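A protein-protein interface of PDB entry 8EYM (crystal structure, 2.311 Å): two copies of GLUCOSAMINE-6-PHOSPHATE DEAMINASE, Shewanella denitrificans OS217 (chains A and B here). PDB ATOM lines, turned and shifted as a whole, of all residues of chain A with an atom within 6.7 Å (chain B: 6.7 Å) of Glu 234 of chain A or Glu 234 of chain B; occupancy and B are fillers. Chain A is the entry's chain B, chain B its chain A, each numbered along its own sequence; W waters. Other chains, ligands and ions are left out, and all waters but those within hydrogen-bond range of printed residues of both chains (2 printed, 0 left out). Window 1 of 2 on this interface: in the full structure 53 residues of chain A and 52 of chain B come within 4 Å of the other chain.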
ATOM      1  N   ASN A 205     -32.084  19.663  -4.805  1.00  0.00           N
ATOM      2  CA  ASN A 205     -30.868  19.574  -5.597  1.00  0.00           C
ATOM      3  C   ASN A 205     -30.448  20.984  -5.979  1.00  0.00           C
ATOM      4  O   ASN A 205     -31.279  21.889  -6.079  1.00  0.00           O
ATOM      5  CB  ASN A 205     -31.097  18.743  -6.864  1.00  0.00           C
ATOM      6  CG  ASN A 205     -32.162  19.343  -7.755  1.00  0.00           C
ATOM      7  OD1 ASN A 205     -33.350  19.304  -7.433  1.00  0.00           O
ATOM      8  ND2 ASN A 205     -31.741  19.934  -8.860  1.00  0.00           N
ATOM      9  N   LEU A 206     -29.152  21.162  -6.220  1.00  0.00           N
ATOM     10  CA  LEU A 206     -28.629  22.471  -6.591  1.00  0.00           C
ATOM     11  C   LEU A 206     -27.320  22.279  -7.331  1.00  0.00           C
ATOM     12  O   LEU A 206     -26.755  21.183  -7.362  1.00  0.00           O
ATOM     13  CB  LEU A 206     -28.401  23.376  -5.369  1.00  0.00           C
ATOM     14  CG  LEU A 206     -27.457  22.961  -4.234  1.00  0.00           C
ATOM     15  CD1 LEU A 206     -26.012  23.199  -4.589  1.00  0.00           C
ATOM     16  CD2 LEU A 206     -27.770  23.791  -3.008  1.00  0.00           C
ATOM     17  N   VAL A 207     -26.812  23.382  -7.878  1.00  0.00           N
ATOM     18  CA  VAL A 207     -25.554  23.382  -8.603  1.00  0.00           C
ATOM     19  C   VAL A 207     -24.580  24.297  -7.869  1.00  0.00           C
ATOM     20  O   VAL A 207     -24.945  25.391  -7.428  1.00  0.00           O
ATOM     21  CB  VAL A 207     -25.766  23.833 -10.070  1.00  0.00           C
ATOM     22  CG1 VAL A 207     -24.463  24.219 -10.717  1.00  0.00           C
ATOM     23  CG2 VAL A 207     -26.453  22.743 -10.873  1.00  0.00           C
ATOM     24  N   VAL A 208     -23.349  23.836  -7.709  1.00  0.00           N
ATOM     25  CA  VAL A 208     -22.272  24.668  -7.196  1.00  0.00           C
ATOM     26  C   VAL A 208     -21.437  25.090  -8.397  1.00  0.00           C
ATOM     27  O   VAL A 208     -20.999  24.237  -9.176  1.00  0.00           O
ATOM     28  CB  VAL A 208     -21.437  23.902  -6.161  1.00  0.00           C
ATOM     29  CG1 VAL A 208     -20.449  24.837  -5.470  1.00  0.00           C
ATOM     30  CG2 VAL A 208     -22.358  23.205  -5.142  1.00  0.00           C
ATOM     31  N   LEU A 209     -21.285  26.403  -8.591  1.00  0.00           N
ATOM     32  CA  LEU A 209     -20.502  26.972  -9.692  1.00  0.00           C
ATOM     33  C   LEU A 209     -19.253  27.672  -9.172  1.00  0.00           C
ATOM     34  O   LEU A 209     -19.334  28.530  -8.283  1.00  0.00           O
ATOM     35  CB  LEU A 209     -21.300  27.998 -10.512  1.00  0.00           C
ATOM     36  CG  LEU A 209     -22.368  27.501 -11.476  1.00  0.00           C
ATOM     37  CD1 LEU A 209     -22.809  28.655 -12.365  1.00  0.00           C
ATOM     38  CD2 LEU A 209     -21.832  26.370 -12.313  1.00  0.00           C
ATOM     39  N   SER A 218     -15.391  23.752  -5.068  1.00  0.00           N
ATOM     40  CA  SER A 218     -16.814  23.516  -5.310  1.00  0.00           C
ATOM     41  C   SER A 218     -17.152  22.036  -5.216  1.00  0.00           C
ATOM     42  O   SER A 218     -18.222  21.675  -4.707  1.00  0.00           O
ATOM     43  CB  SER A 218     -17.217  24.043  -6.684  1.00  0.00           C
ATOM     44  OG  SER A 218     -17.392  25.445  -6.661  1.00  0.00           O
ATOM     45  N   ALA A 222     -19.944  20.492  -2.771  1.00  0.00           N
ATOM     46  CA  ALA A 222     -21.063  19.681  -3.259  1.00  0.00           C
ATOM     47  C   ALA A 222     -21.134  18.344  -2.529  1.00  0.00           C
ATOM     48  O   ALA A 222     -22.231  17.835  -2.250  1.00  0.00           O
ATOM     49  CB  ALA A 222     -20.976  19.486  -4.777  1.00  0.00           C
ATOM     50  N   LEU A 225     -22.596  18.965   0.949  1.00  0.00           N
ATOM     51  CA  LEU A 225     -24.041  19.157   0.907  1.00  0.00           C
ATOM     52  C   LEU A 225     -24.764  17.826   0.738  1.00  0.00           C
ATOM     53  O   LEU A 225     -25.820  17.621   1.333  1.00  0.00           O
ATOM     54  CB  LEU A 225     -24.405  20.122  -0.213  1.00  0.00           C
ATOM     55  CG  LEU A 225     -23.959  21.569  -0.005  1.00  0.00           C
ATOM     56  CD1 LEU A 225     -23.881  22.283  -1.356  1.00  0.00           C
ATOM     57  CD2 LEU A 225     -24.892  22.294   0.952  1.00  0.00           C
ATOM     58  N   LYS A 226     -24.238  16.922  -0.102  1.00  0.00           N
ATOM     59  CA  LYS A 226     -24.791  15.567  -0.148  1.00  0.00           C
ATOM     60  C   LYS A 226     -24.629  14.879   1.201  1.00  0.00           C
ATOM     61  O   LYS A 226     -25.580  14.300   1.739  1.00  0.00           O
ATOM     62  CB  LYS A 226     -24.091  14.711  -1.210  1.00  0.00           C
ATOM     63  CG  LYS A 226     -24.287  15.080  -2.660  1.00  0.00           C
ATOM     64  CD  LYS A 226     -23.621  14.002  -3.532  1.00  0.00           C
ATOM     65  CE  LYS A 226     -23.755  14.304  -5.000  1.00  0.00           C
ATOM     66  NZ  LYS A 226     -22.693  15.293  -5.426  1.00  0.00           N
ATOM     67  N   ILE A 231     -28.686  16.979   0.354  1.00  0.00           N
ATOM     68  CA  ILE A 231     -29.052  17.749  -0.834  1.00  0.00           C
ATOM     69  C   ILE A 231     -28.260  17.209  -2.015  1.00  0.00           C
ATOM     70  O   ILE A 231     -27.044  17.001  -1.905  1.00  0.00           O
ATOM     71  CB  ILE A 231     -28.759  19.244  -0.639  1.00  0.00           C
ATOM     72  CG1 ILE A 231     -29.650  19.824   0.457  1.00  0.00           C
ATOM     73  CG2 ILE A 231     -28.946  19.997  -1.954  1.00  0.00           C
ATOM     74  CD1 ILE A 231     -29.232  21.204   0.884  1.00  0.00           C
ATOM     75  N   HIS A 232     -28.937  16.986  -3.148  1.00  0.00           N
ATOM     76  CA  HIS A 232     -28.243  16.552  -4.363  1.00  0.00           C
ATOM     77  C   HIS A 232     -27.558  17.756  -5.007  1.00  0.00           C
ATOM     78  O   HIS A 232     -28.069  18.385  -5.932  1.00  0.00           O
ATOM     79  CB  HIS A 232     -29.191  15.887  -5.348  1.00  0.00           C
ATOM     80  CG  HIS A 232     -28.485  15.263  -6.510  1.00  0.00           C
ATOM     81  ND1 HIS A 232     -29.109  14.419  -7.403  1.00  0.00           N
ATOM     82  CD2 HIS A 232     -27.184  15.321  -6.894  1.00  0.00           C
ATOM     83  CE1 HIS A 232     -28.233  14.020  -8.310  1.00  0.00           C
ATOM     84  NE2 HIS A 232     -27.055  14.539  -8.011  1.00  0.00           N
ATOM     85  N   ALA A 233     -26.361  18.063  -4.523  1.00  0.00           N
ATOM     86  CA  ALA A 233     -25.568  19.171  -5.026  1.00  0.00           C
ATOM     87  C   ALA A 233     -24.534  18.632  -6.007  1.00  0.00           C
ATOM     88  O   ALA A 233     -23.887  17.614  -5.735  1.00  0.00           O
ATOM     89  CB  ALA A 233     -24.864  19.852  -3.861  1.00  0.00           C
ATOM     90  N   GLU A 234     -24.403  19.295  -7.155  1.00  0.00           N
ATOM     91  CA  GLU A 234     -23.432  18.920  -8.183  1.00  0.00           C
ATOM     92  C   GLU A 234     -22.585  20.134  -8.569  1.00  0.00           C
ATOM     93  O   GLU A 234     -23.121  21.225  -8.804  1.00  0.00           O
ATOM     94  CB  GLU A 234     -24.104  18.305  -9.424  1.00  0.00           C
ATOM     95  CG  GLU A 234     -23.106  17.835 -10.492  1.00  0.00           C
ATOM     96  CD  GLU A 234     -23.743  17.106 -11.694  1.00  0.00           C
ATOM     97  OE1 GLU A 234     -24.993  17.118 -11.857  1.00  0.00           O
ATOM     98  OE2 GLU A 234     -22.975  16.530 -12.496  1.00  0.00           O
ATOM     99  N   ALA A 235     -21.266  19.938  -8.623  1.00  0.00           N
ATOM    100  CA  ALA A 235     -20.323  21.006  -8.931  1.00  0.00           C
ATOM    101  C   ALA A 235     -20.001  21.052 -10.425  1.00  0.00           C
ATOM    102  O   ALA A 235     -19.703  20.020 -11.042  1.00  0.00           O
ATOM    103  CB  ALA A 235     -19.041  20.813  -8.128  1.00  0.00           C
ATOM    104  N   PHE A 236     -20.023  22.259 -10.989  1.00  0.00           N
ATOM    105  CA  PHE A 236     -19.666  22.495 -12.379  1.00  0.00           C
ATOM    106  C   PHE A 236     -18.699  23.665 -12.452  1.00  0.00           C
ATOM    107  O   PHE A 236     -18.744  24.583 -11.627  1.00  0.00           O
ATOM    108  CB  PHE A 236     -20.901  22.850 -13.215  1.00  0.00           C
ATOM    109  CG  PHE A 236     -21.707  21.664 -13.620  1.00  0.00           C
ATOM    110  CD1 PHE A 236     -21.332  20.894 -14.704  1.00  0.00           C
ATOM    111  CD2 PHE A 236     -22.817  21.284 -12.883  1.00  0.00           C
ATOM    112  CE1 PHE A 236     -22.065  19.782 -15.066  1.00  0.00           C
ATOM    113  CE2 PHE A 236     -23.560  20.172 -13.242  1.00  0.00           C
ATOM    114  CZ  PHE A 236     -23.186  19.418 -14.344  1.00  0.00           C
ATOM    115  N   PHE A 241     -20.571  24.648 -17.504  1.00  0.00           N
ATOM    116  CA  PHE A 241     -22.009  24.611 -17.253  1.00  0.00           C
ATOM    117  C   PHE A 241     -22.827  24.963 -18.491  1.00  0.00           C
ATOM    118  O   PHE A 241     -23.935  24.436 -18.676  1.00  0.00           O
ATOM    119  CB  PHE A 241     -22.349  25.558 -16.099  1.00  0.00           C
ATOM    120  CG  PHE A 241     -23.741  25.383 -15.546  1.00  0.00           C
ATOM    121  CD1 PHE A 241     -24.125  24.186 -14.952  1.00  0.00           C
ATOM    122  CD2 PHE A 241     -24.648  26.433 -15.565  1.00  0.00           C
ATOM    123  CE1 PHE A 241     -25.397  24.027 -14.412  1.00  0.00           C
ATOM    124  CE2 PHE A 241     -25.930  26.276 -15.029  1.00  0.00           C
ATOM    125  CZ  PHE A 241     -26.298  25.070 -14.450  1.00  0.00           C
ATOM    126  N   PRO A 245     -25.574  21.494 -19.259  1.00  0.00           N
ATOM    127  CA  PRO A 245     -26.198  21.521 -17.920  1.00  0.00           C
ATOM    128  C   PRO A 245     -27.025  22.766 -17.644  1.00  0.00           C
ATOM    129  O   PRO A 245     -27.959  22.711 -16.835  1.00  0.00           O
ATOM    130  CB  PRO A 245     -25.001  21.392 -16.972  1.00  0.00           C
ATOM    131  CG  PRO A 245     -23.986  20.641 -17.777  1.00  0.00           C
ATOM    132  CD  PRO A 245     -24.147  21.140 -19.184  1.00  0.00           C
ATOM    133  N   LEU A 248     -30.913  23.164 -16.960  1.00  0.00           N
ATOM    134  CA  LEU A 248     -31.642  23.058 -15.696  1.00  0.00           C
ATOM    135  C   LEU A 248     -32.169  24.405 -15.206  1.00  0.00           C
ATOM    136  O   LEU A 248     -33.044  24.437 -14.336  1.00  0.00           O
ATOM    137  CB  LEU A 248     -30.750  22.412 -14.632  1.00  0.00           C
ATOM    138  CG  LEU A 248     -30.336  20.959 -14.913  1.00  0.00           C
ATOM    139  CD1 LEU A 248     -29.184  20.538 -14.031  1.00  0.00           C
ATOM    140  CD2 LEU A 248     -31.502  19.999 -14.742  1.00  0.00           C
ATOM    141  N   ASN B 205     -34.461  14.780  -9.899  1.00  0.00           N
ATOM    142  CA  ASN B 205     -33.029  14.544  -9.911  1.00  0.00           C
ATOM    143  C   ASN B 205     -32.792  13.052  -9.750  1.00  0.00           C
ATOM    144  O   ASN B 205     -33.640  12.324  -9.224  1.00  0.00           O
ATOM    145  CB  ASN B 205     -32.331  15.269  -8.765  1.00  0.00           C
ATOM    146  CG  ASN B 205     -32.800  14.783  -7.413  1.00  0.00           C
ATOM    147  OD1 ASN B 205     -33.928  15.059  -6.997  1.00  0.00           O
ATOM    148  ND2 ASN B 205     -31.938  14.042  -6.718  1.00  0.00           N
ATOM    149  N   LEU B 206     -31.628  12.596 -10.218  1.00  0.00           N
ATOM    150  CA  LEU B 206     -31.283  11.186 -10.079  1.00  0.00           C
ATOM    151  C   LEU B 206     -29.773  11.003 -10.193  1.00  0.00           C
ATOM    152  O   LEU B 206     -29.027  11.924 -10.545  1.00  0.00           O
ATOM    153  CB  LEU B 206     -32.052  10.309 -11.081  1.00  0.00           C
ATOM    154  CG  LEU B 206     -31.866  10.567 -12.575  1.00  0.00           C
ATOM    155  CD1 LEU B 206     -30.596   9.891 -13.094  1.00  0.00           C
ATOM    156  CD2 LEU B 206     -33.083  10.050 -13.336  1.00  0.00           C
ATOM    157  N   VAL B 207     -29.345   9.774  -9.930  1.00  0.00           N
ATOM    158  CA  VAL B 207     -27.948   9.363 -10.013  1.00  0.00           C
ATOM    159  C   VAL B 207     -27.822   8.256 -11.060  1.00  0.00           C
ATOM    160  O   VAL B 207     -28.665   7.358 -11.137  1.00  0.00           O
ATOM    161  CB  VAL B 207     -27.435   8.912  -8.627  1.00  0.00           C
ATOM    162  CG1 VAL B 207     -26.156   8.144  -8.742  1.00  0.00           C
ATOM    163  CG2 VAL B 207     -27.268  10.118  -7.695  1.00  0.00           C
ATOM    164  N   VAL B 208     -26.804   8.363 -11.910  1.00  0.00           N
ATOM    165  CA  VAL B 208     -26.437   7.316 -12.856  1.00  0.00           C
ATOM    166  C   VAL B 208     -25.209   6.637 -12.272  1.00  0.00           C
ATOM    167  O   VAL B 208     -24.207   7.300 -11.995  1.00  0.00           O
ATOM    168  CB  VAL B 208     -26.144   7.918 -14.239  1.00  0.00           C
ATOM    169  CG1 VAL B 208     -25.988   6.840 -15.287  1.00  0.00           C
ATOM    170  CG2 VAL B 208     -27.237   8.912 -14.618  1.00  0.00           C
ATOM    171  N   LEU B 209     -25.273   5.330 -12.050  1.00  0.00           N
ATOM    172  CA  LEU B 209     -24.161   4.596 -11.453  1.00  0.00           C
ATOM    173  C   LEU B 209     -23.557   3.661 -12.489  1.00  0.00           C
ATOM    174  O   LEU B 209     -24.289   2.927 -13.165  1.00  0.00           O
ATOM    175  CB  LEU B 209     -24.615   3.766 -10.246  1.00  0.00           C
ATOM    176  CG  LEU B 209     -24.991   4.495  -8.947  1.00  0.00           C
ATOM    177  CD1 LEU B 209     -25.147   3.511  -7.778  1.00  0.00           C
ATOM    178  CD2 LEU B 209     -23.970   5.574  -8.611  1.00  0.00           C
ATOM    179  N   SER B 218     -21.729   6.647 -18.324  1.00  0.00           N
ATOM    180  CA  SER B 218     -22.665   7.258 -17.381  1.00  0.00           C
ATOM    181  C   SER B 218     -22.614   8.776 -17.448  1.00  0.00           C
ATOM    182  O   SER B 218     -23.652   9.439 -17.350  1.00  0.00           O
ATOM    183  CB  SER B 218     -22.341   6.809 -15.962  1.00  0.00           C
ATOM    184  OG  SER B 218     -22.862   5.528 -15.722  1.00  0.00           O
ATOM    185  N   ALA B 222     -25.770  11.003 -18.111  1.00  0.00           N
ATOM    186  CA  ALA B 222     -26.146  12.054 -17.137  1.00  0.00           C
ATOM    187  C   ALA B 222     -26.315  13.396 -17.858  1.00  0.00           C
ATOM    188  O   ALA B 222     -27.305  14.091 -17.574  1.00  0.00           O
ATOM    189  CB  ALA B 222     -25.101  12.137 -16.053  1.00  0.00           C
ATOM    190  N   LEU B 225     -29.578  13.407 -19.887  1.00  0.00           N
ATOM    191  CA  LEU B 225     -30.778  13.536 -19.016  1.00  0.00           C
ATOM    192  C   LEU B 225     -30.988  15.018 -18.687  1.00  0.00           C
ATOM    193  O   LEU B 225     -32.142  15.476 -18.762  1.00  0.00           O
ATOM    194  CB  LEU B 225     -30.574  12.689 -17.758  1.00  0.00           C
ATOM    195  CG  LEU B 225     -30.706  11.183 -17.974  1.00  0.00           C
ATOM    196  CD1 LEU B 225     -30.303  10.411 -16.728  1.00  0.00           C
ATOM    197  CD2 LEU B 225     -32.122  10.821 -18.393  1.00  0.00           C
ATOM    198  N   LYS B 226     -29.909  15.739 -18.370  1.00  0.00           N
ATOM    199  CA  LYS B 226     -30.002  17.177 -18.149  1.00  0.00           C
ATOM    200  C   LYS B 226     -30.446  17.890 -19.418  1.00  0.00           C
ATOM    201  O   LYS B 226     -31.370  18.713 -19.402  1.00  0.00           O
ATOM    202  CB  LYS B 226     -28.642  17.719 -17.728  1.00  0.00           C
ATOM    203  CG  LYS B 226     -28.134  17.285 -16.376  1.00  0.00           C
ATOM    204  CD  LYS B 226     -26.865  18.062 -16.091  1.00  0.00           C
ATOM    205  CE  LYS B 226     -26.312  17.787 -14.704  1.00  0.00           C
ATOM    206  NZ  LYS B 226     -25.496  16.556 -14.649  1.00  0.00           N
ATOM    207  N   ILE B 231     -33.729  16.811 -16.337  1.00  0.00           N
ATOM    208  CA  ILE B 231     -33.548  16.096 -15.081  1.00  0.00           C
ATOM    209  C   ILE B 231     -32.133  16.368 -14.564  1.00  0.00           C
ATOM    210  O   ILE B 231     -31.148  16.269 -15.312  1.00  0.00           O
ATOM    211  CB  ILE B 231     -33.806  14.591 -15.267  1.00  0.00           C
ATOM    212  CG1 ILE B 231     -35.289  14.346 -15.597  1.00  0.00           C
ATOM    213  CG2 ILE B 231     -33.406  13.823 -14.028  1.00  0.00           C
ATOM    214  CD1 ILE B 231     -35.614  12.939 -16.080  1.00  0.00           C
ATOM    215  N   HIS B 232     -32.025  16.724 -13.285  1.00  0.00           N
ATOM    216  CA  HIS B 232     -30.712  16.882 -12.679  1.00  0.00           C
ATOM    217  C   HIS B 232     -30.155  15.497 -12.378  1.00  0.00           C
ATOM    218  O   HIS B 232     -30.244  14.988 -11.261  1.00  0.00           O
ATOM    219  CB  HIS B 232     -30.762  17.741 -11.428  1.00  0.00           C
ATOM    220  CG  HIS B 232     -29.405  18.061 -10.890  1.00  0.00           C
ATOM    221  ND1 HIS B 232     -29.187  19.044  -9.951  1.00  0.00           N
ATOM    222  CD2 HIS B 232     -28.191  17.527 -11.168  1.00  0.00           C
ATOM    223  CE1 HIS B 232     -27.897  19.100  -9.671  1.00  0.00           C
ATOM    224  NE2 HIS B 232     -27.271  18.191 -10.400  1.00  0.00           N
ATOM    225  N   ALA B 233     -29.543  14.899 -13.399  1.00  0.00           N
ATOM    226  CA  ALA B 233     -28.922  13.585 -13.306  1.00  0.00           C
ATOM    227  C   ALA B 233     -27.418  13.764 -13.117  1.00  0.00           C
ATOM    228  O   ALA B 233     -26.790  14.572 -13.818  1.00  0.00           O
ATOM    229  CB  ALA B 233     -29.181  12.806 -14.597  1.00  0.00           C
ATOM    230  N   GLU B 234     -26.842  13.006 -12.183  1.00  0.00           N
ATOM    231  CA  GLU B 234     -25.415  13.068 -11.899  1.00  0.00           C
ATOM    232  C   GLU B 234     -24.812  11.667 -11.959  1.00  0.00           C
ATOM    233  O   GLU B 234     -25.346  10.734 -11.348  1.00  0.00           O
ATOM    234  CB  GLU B 234     -25.136  13.705 -10.531  1.00  0.00           C
ATOM    235  CG  GLU B 234     -23.638  13.865 -10.275  1.00  0.00           C
ATOM    236  CD  GLU B 234     -23.306  14.596  -8.972  1.00  0.00           C
ATOM    237  OE1 GLU B 234     -24.206  14.755  -8.121  1.00  0.00           O
ATOM    238  OE2 GLU B 234     -22.139  15.033  -8.817  1.00  0.00           O
ATOM    239  N   ALA B 235     -23.683  11.535 -12.669  1.00  0.00           N
ATOM    240  CA  ALA B 235     -23.013  10.256 -12.864  1.00  0.00           C
ATOM    241  C   ALA B 235     -21.976  10.029 -11.773  1.00  0.00           C
ATOM    242  O   ALA B 235     -21.208  10.936 -11.435  1.00  0.00           O
ATOM    243  CB  ALA B 235     -22.315  10.204 -14.224  1.00  0.00           C
ATOM    244  N   PHE B 236     -21.965   8.820 -11.224  1.00  0.00           N
ATOM    245  CA  PHE B 236     -20.974   8.416 -10.247  1.00  0.00           C
ATOM    246  C   PHE B 236     -20.422   7.041 -10.577  1.00  0.00           C
ATOM    247  O   PHE B 236     -21.137   6.157 -11.051  1.00  0.00           O
ATOM    248  CB  PHE B 236     -21.579   8.324  -8.852  1.00  0.00           C
ATOM    249  CG  PHE B 236     -21.677   9.631  -8.160  1.00  0.00           C
ATOM    250  CD1 PHE B 236     -20.561  10.182  -7.551  1.00  0.00           C
ATOM    251  CD2 PHE B 236     -22.878  10.310  -8.101  1.00  0.00           C
ATOM    252  CE1 PHE B 236     -20.642  11.401  -6.892  1.00  0.00           C
ATOM    253  CE2 PHE B 236     -22.969  11.537  -7.449  1.00  0.00           C
ATOM    254  CZ  PHE B 236     -21.852  12.086  -6.850  1.00  0.00           C
ATOM    255  N   LEU B 248     -27.752  10.053   0.101  1.00  0.00           N
ATOM    256  CA  LEU B 248     -28.949  10.522  -0.588  1.00  0.00           C
ATOM    257  C   LEU B 248     -29.972   9.414  -0.800  1.00  0.00           C
ATOM    258  O   LEU B 248     -31.125   9.711  -1.138  1.00  0.00           O
ATOM    259  CB  LEU B 248     -28.605  11.105  -1.955  1.00  0.00           C
ATOM    260  CG  LEU B 248     -27.771  12.370  -2.043  1.00  0.00           C
ATOM    261  CD1 LEU B 248     -27.277  12.557  -3.480  1.00  0.00           C
ATOM    262  CD2 LEU B 248     -28.617  13.545  -1.601  1.00  0.00           C
HETATM  263  O   HOH W   1     -20.473  17.272  -7.819  1.00  0.00           O
HETATM  264  O   HOH W   2     -22.761  13.988 -14.145  1.00  0.00           O
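A ring nitrogen (ND1) of His 232 of chain A sits at hydrogen-bond distance from the side-chain amide nitrogen (ND2) of Asn 205 of chain B. The side-chain amino group of Lys 226 of chain B is in salt-bridge range of the side-chain carboxylate of Glu 234 of chain A (2.9 Å). The side-chain amide nitrogen (ND2) of Asn 205 of chain A lies within hydrogen-bond range of a ring nitrogen (ND1) of His 232 of chain B, 2.9 Å away. NE2 of His 232 of chain B sits at hydrogen-bond distance from OE1 of Glu 234 of chain A, at 2.9 Å. The side-chain amino group of Lys 226 of chain A lies within salt-bridge range of the side-chain carboxylate of Glu 234 of chain B (3.1 Å). OE1 of Glu 234 of chain B sits at hydrogen-bond distance from NE2 of His 232 of chain A.
The backbone NH of Ile 231 of chain B lies within hydrogen-bond range of the backbone carbonyl oxygen of Leu 225 of chain B (3.2 Å). The backbone carbonyl oxygen (O) of Ala 233 of chain B sits at hydrogen-bond distance from the side-chain amino group (NZ) of Lys 226 of chain B, at 2.5 Å. The backbone NH of Val 208 of chain A sits at hydrogen-bond distance from the backbone carbonyl oxygen of Glu 234 of chain A. The backbone NH (N) of Ile 231 of chain A is in hydrogen-bond range of the backbone carbonyl oxygen (O) of Leu 225 of chain A, 3.1 Å away. The backbone carbonyl oxygen (O) of Ile 231 of chain A sits close to the backbone NH (N) of Lys 226 of chain A (3.3 Å). The side-chain amino group of Lys 226 of chain A sits at hydrogen-bond distance from the backbone carbonyl oxygen of Ala 233 of chain A (2.6 Å).
Leu 206 of chain A touches His 232 of chain B (O to CE1, 3.3 Å). Leu 248 of chain B touches Lys 226 of chain A. CE1 of His 232 of chain A touches O of Leu 206 of chain B (3.2 Å). His 232 of chain B touches His 232 of chain A (O to CE1, 3.7 Å). Leu 248 of chain B touches His 232 of chain A. O of Ala 233 of chain A touches OE1 of Glu 234 of chain B, at 3.7 Å. Ala 233 of chain B touches Glu 234 of chain A. CD of Lys 226 of chain B touches CB of Pro 245 of chain A, at 3.9 Å. CD1 of Leu 248 of chain A touches CD of Lys 226 of chain B, 3.97 Å away. Leu 248 of chain A touches Ile 231 of chain B (CD2 to C, 3.7 Å).
Of chain B, only Lys 226 (2.9 Å), His 232 (2.9 Å), Ala 233 (3.7 Å) and Glu 234 (3.4 Å) come within 4 Å of Glu 234 of chain A. Ala 235 of chain A touches none of the printed residues of chain B. Of the printed residues of chain B, Phe 236 of chain A touches Lys 226. Printed residues of chain B within 4 Å of Leu 248 of chain A: Lys 226 (3.97 Å), Ile 231 (3.7 Å) and His 232 (3.6 Å). Val 207 of chain B touches none of the printed residues of chain A. Printed residues of chain A within 4 Å of Ile 231 of chain B: Leu 248. Glu 234 of chain B touches four residues of chain A. Printed residues of chain A within 4 Å of Phe 236 of chain B: Lys 226. Printed residues of chain A within 4 Å of Leu 248 of chain B: Lys 226 (3.9 Å), Ile 231 (3.7 Å) and His 232 (3.8 Å). The nearest printed residue of chain A that does not touch Leu 248 of chain B is Ala 233 of chain A (5.7 Å).
Hydrophobic or aromatic side chains of chain A that line the printed part of chain B: His 232, Phe 236, Pro 245 and Leu 248. Along chain A the printed residues that touch a printed residue of chain B span positions 205 to 248. Of the 16 printed residues of chain B, 9 touch a printed residue of chain A. Among the printed residues, 21 pairs touch across the chains. Among the printed residues, Asp or Glu carboxylates within 4 Å of a Lys or Arg side-chain nitrogen of the other chain: Lys 226 of chain A with Glu 234 of chain B (3.1 Å) and Glu 234 of chain A with Lys 226 of chain B (2.9 Å).
Ile 231 of chain A touches Leu 248 of chain B, and with the chains exchanged Leu 248 of chain A touches Ile 231 of chain B. His 232 of chain A touches Glu 234 of chain B, and with the chains exchanged Glu 234 of chain A touches His 232 of chain B. His 232 of chain A touches Leu 248 of chain B, and with the chains exchanged Leu 248 of chain A touches His 232 of chain B. Ala 233 of chain A touches Glu 234 of chain B, and with the chains exchanged Glu 234 of chain A touches Ala 233 of chain B. 16 positions are printed for both chains. Of the 21 pairs that touch across the chains among the printed residues, 20 have their exchanged pair printed and touching as well.
Water W1 lies within hydrogen-bond range of N of Ala 235 of chain A (2.9 Å) and OE2 of Glu 234 of chain B (3.0 Å). Water W2 lies within hydrogen-bond range of the backbone NH of Ala 235 of chain B (3.0 Å) and the side-chain carboxylate of Glu 234 of chain A (3.0 Å).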
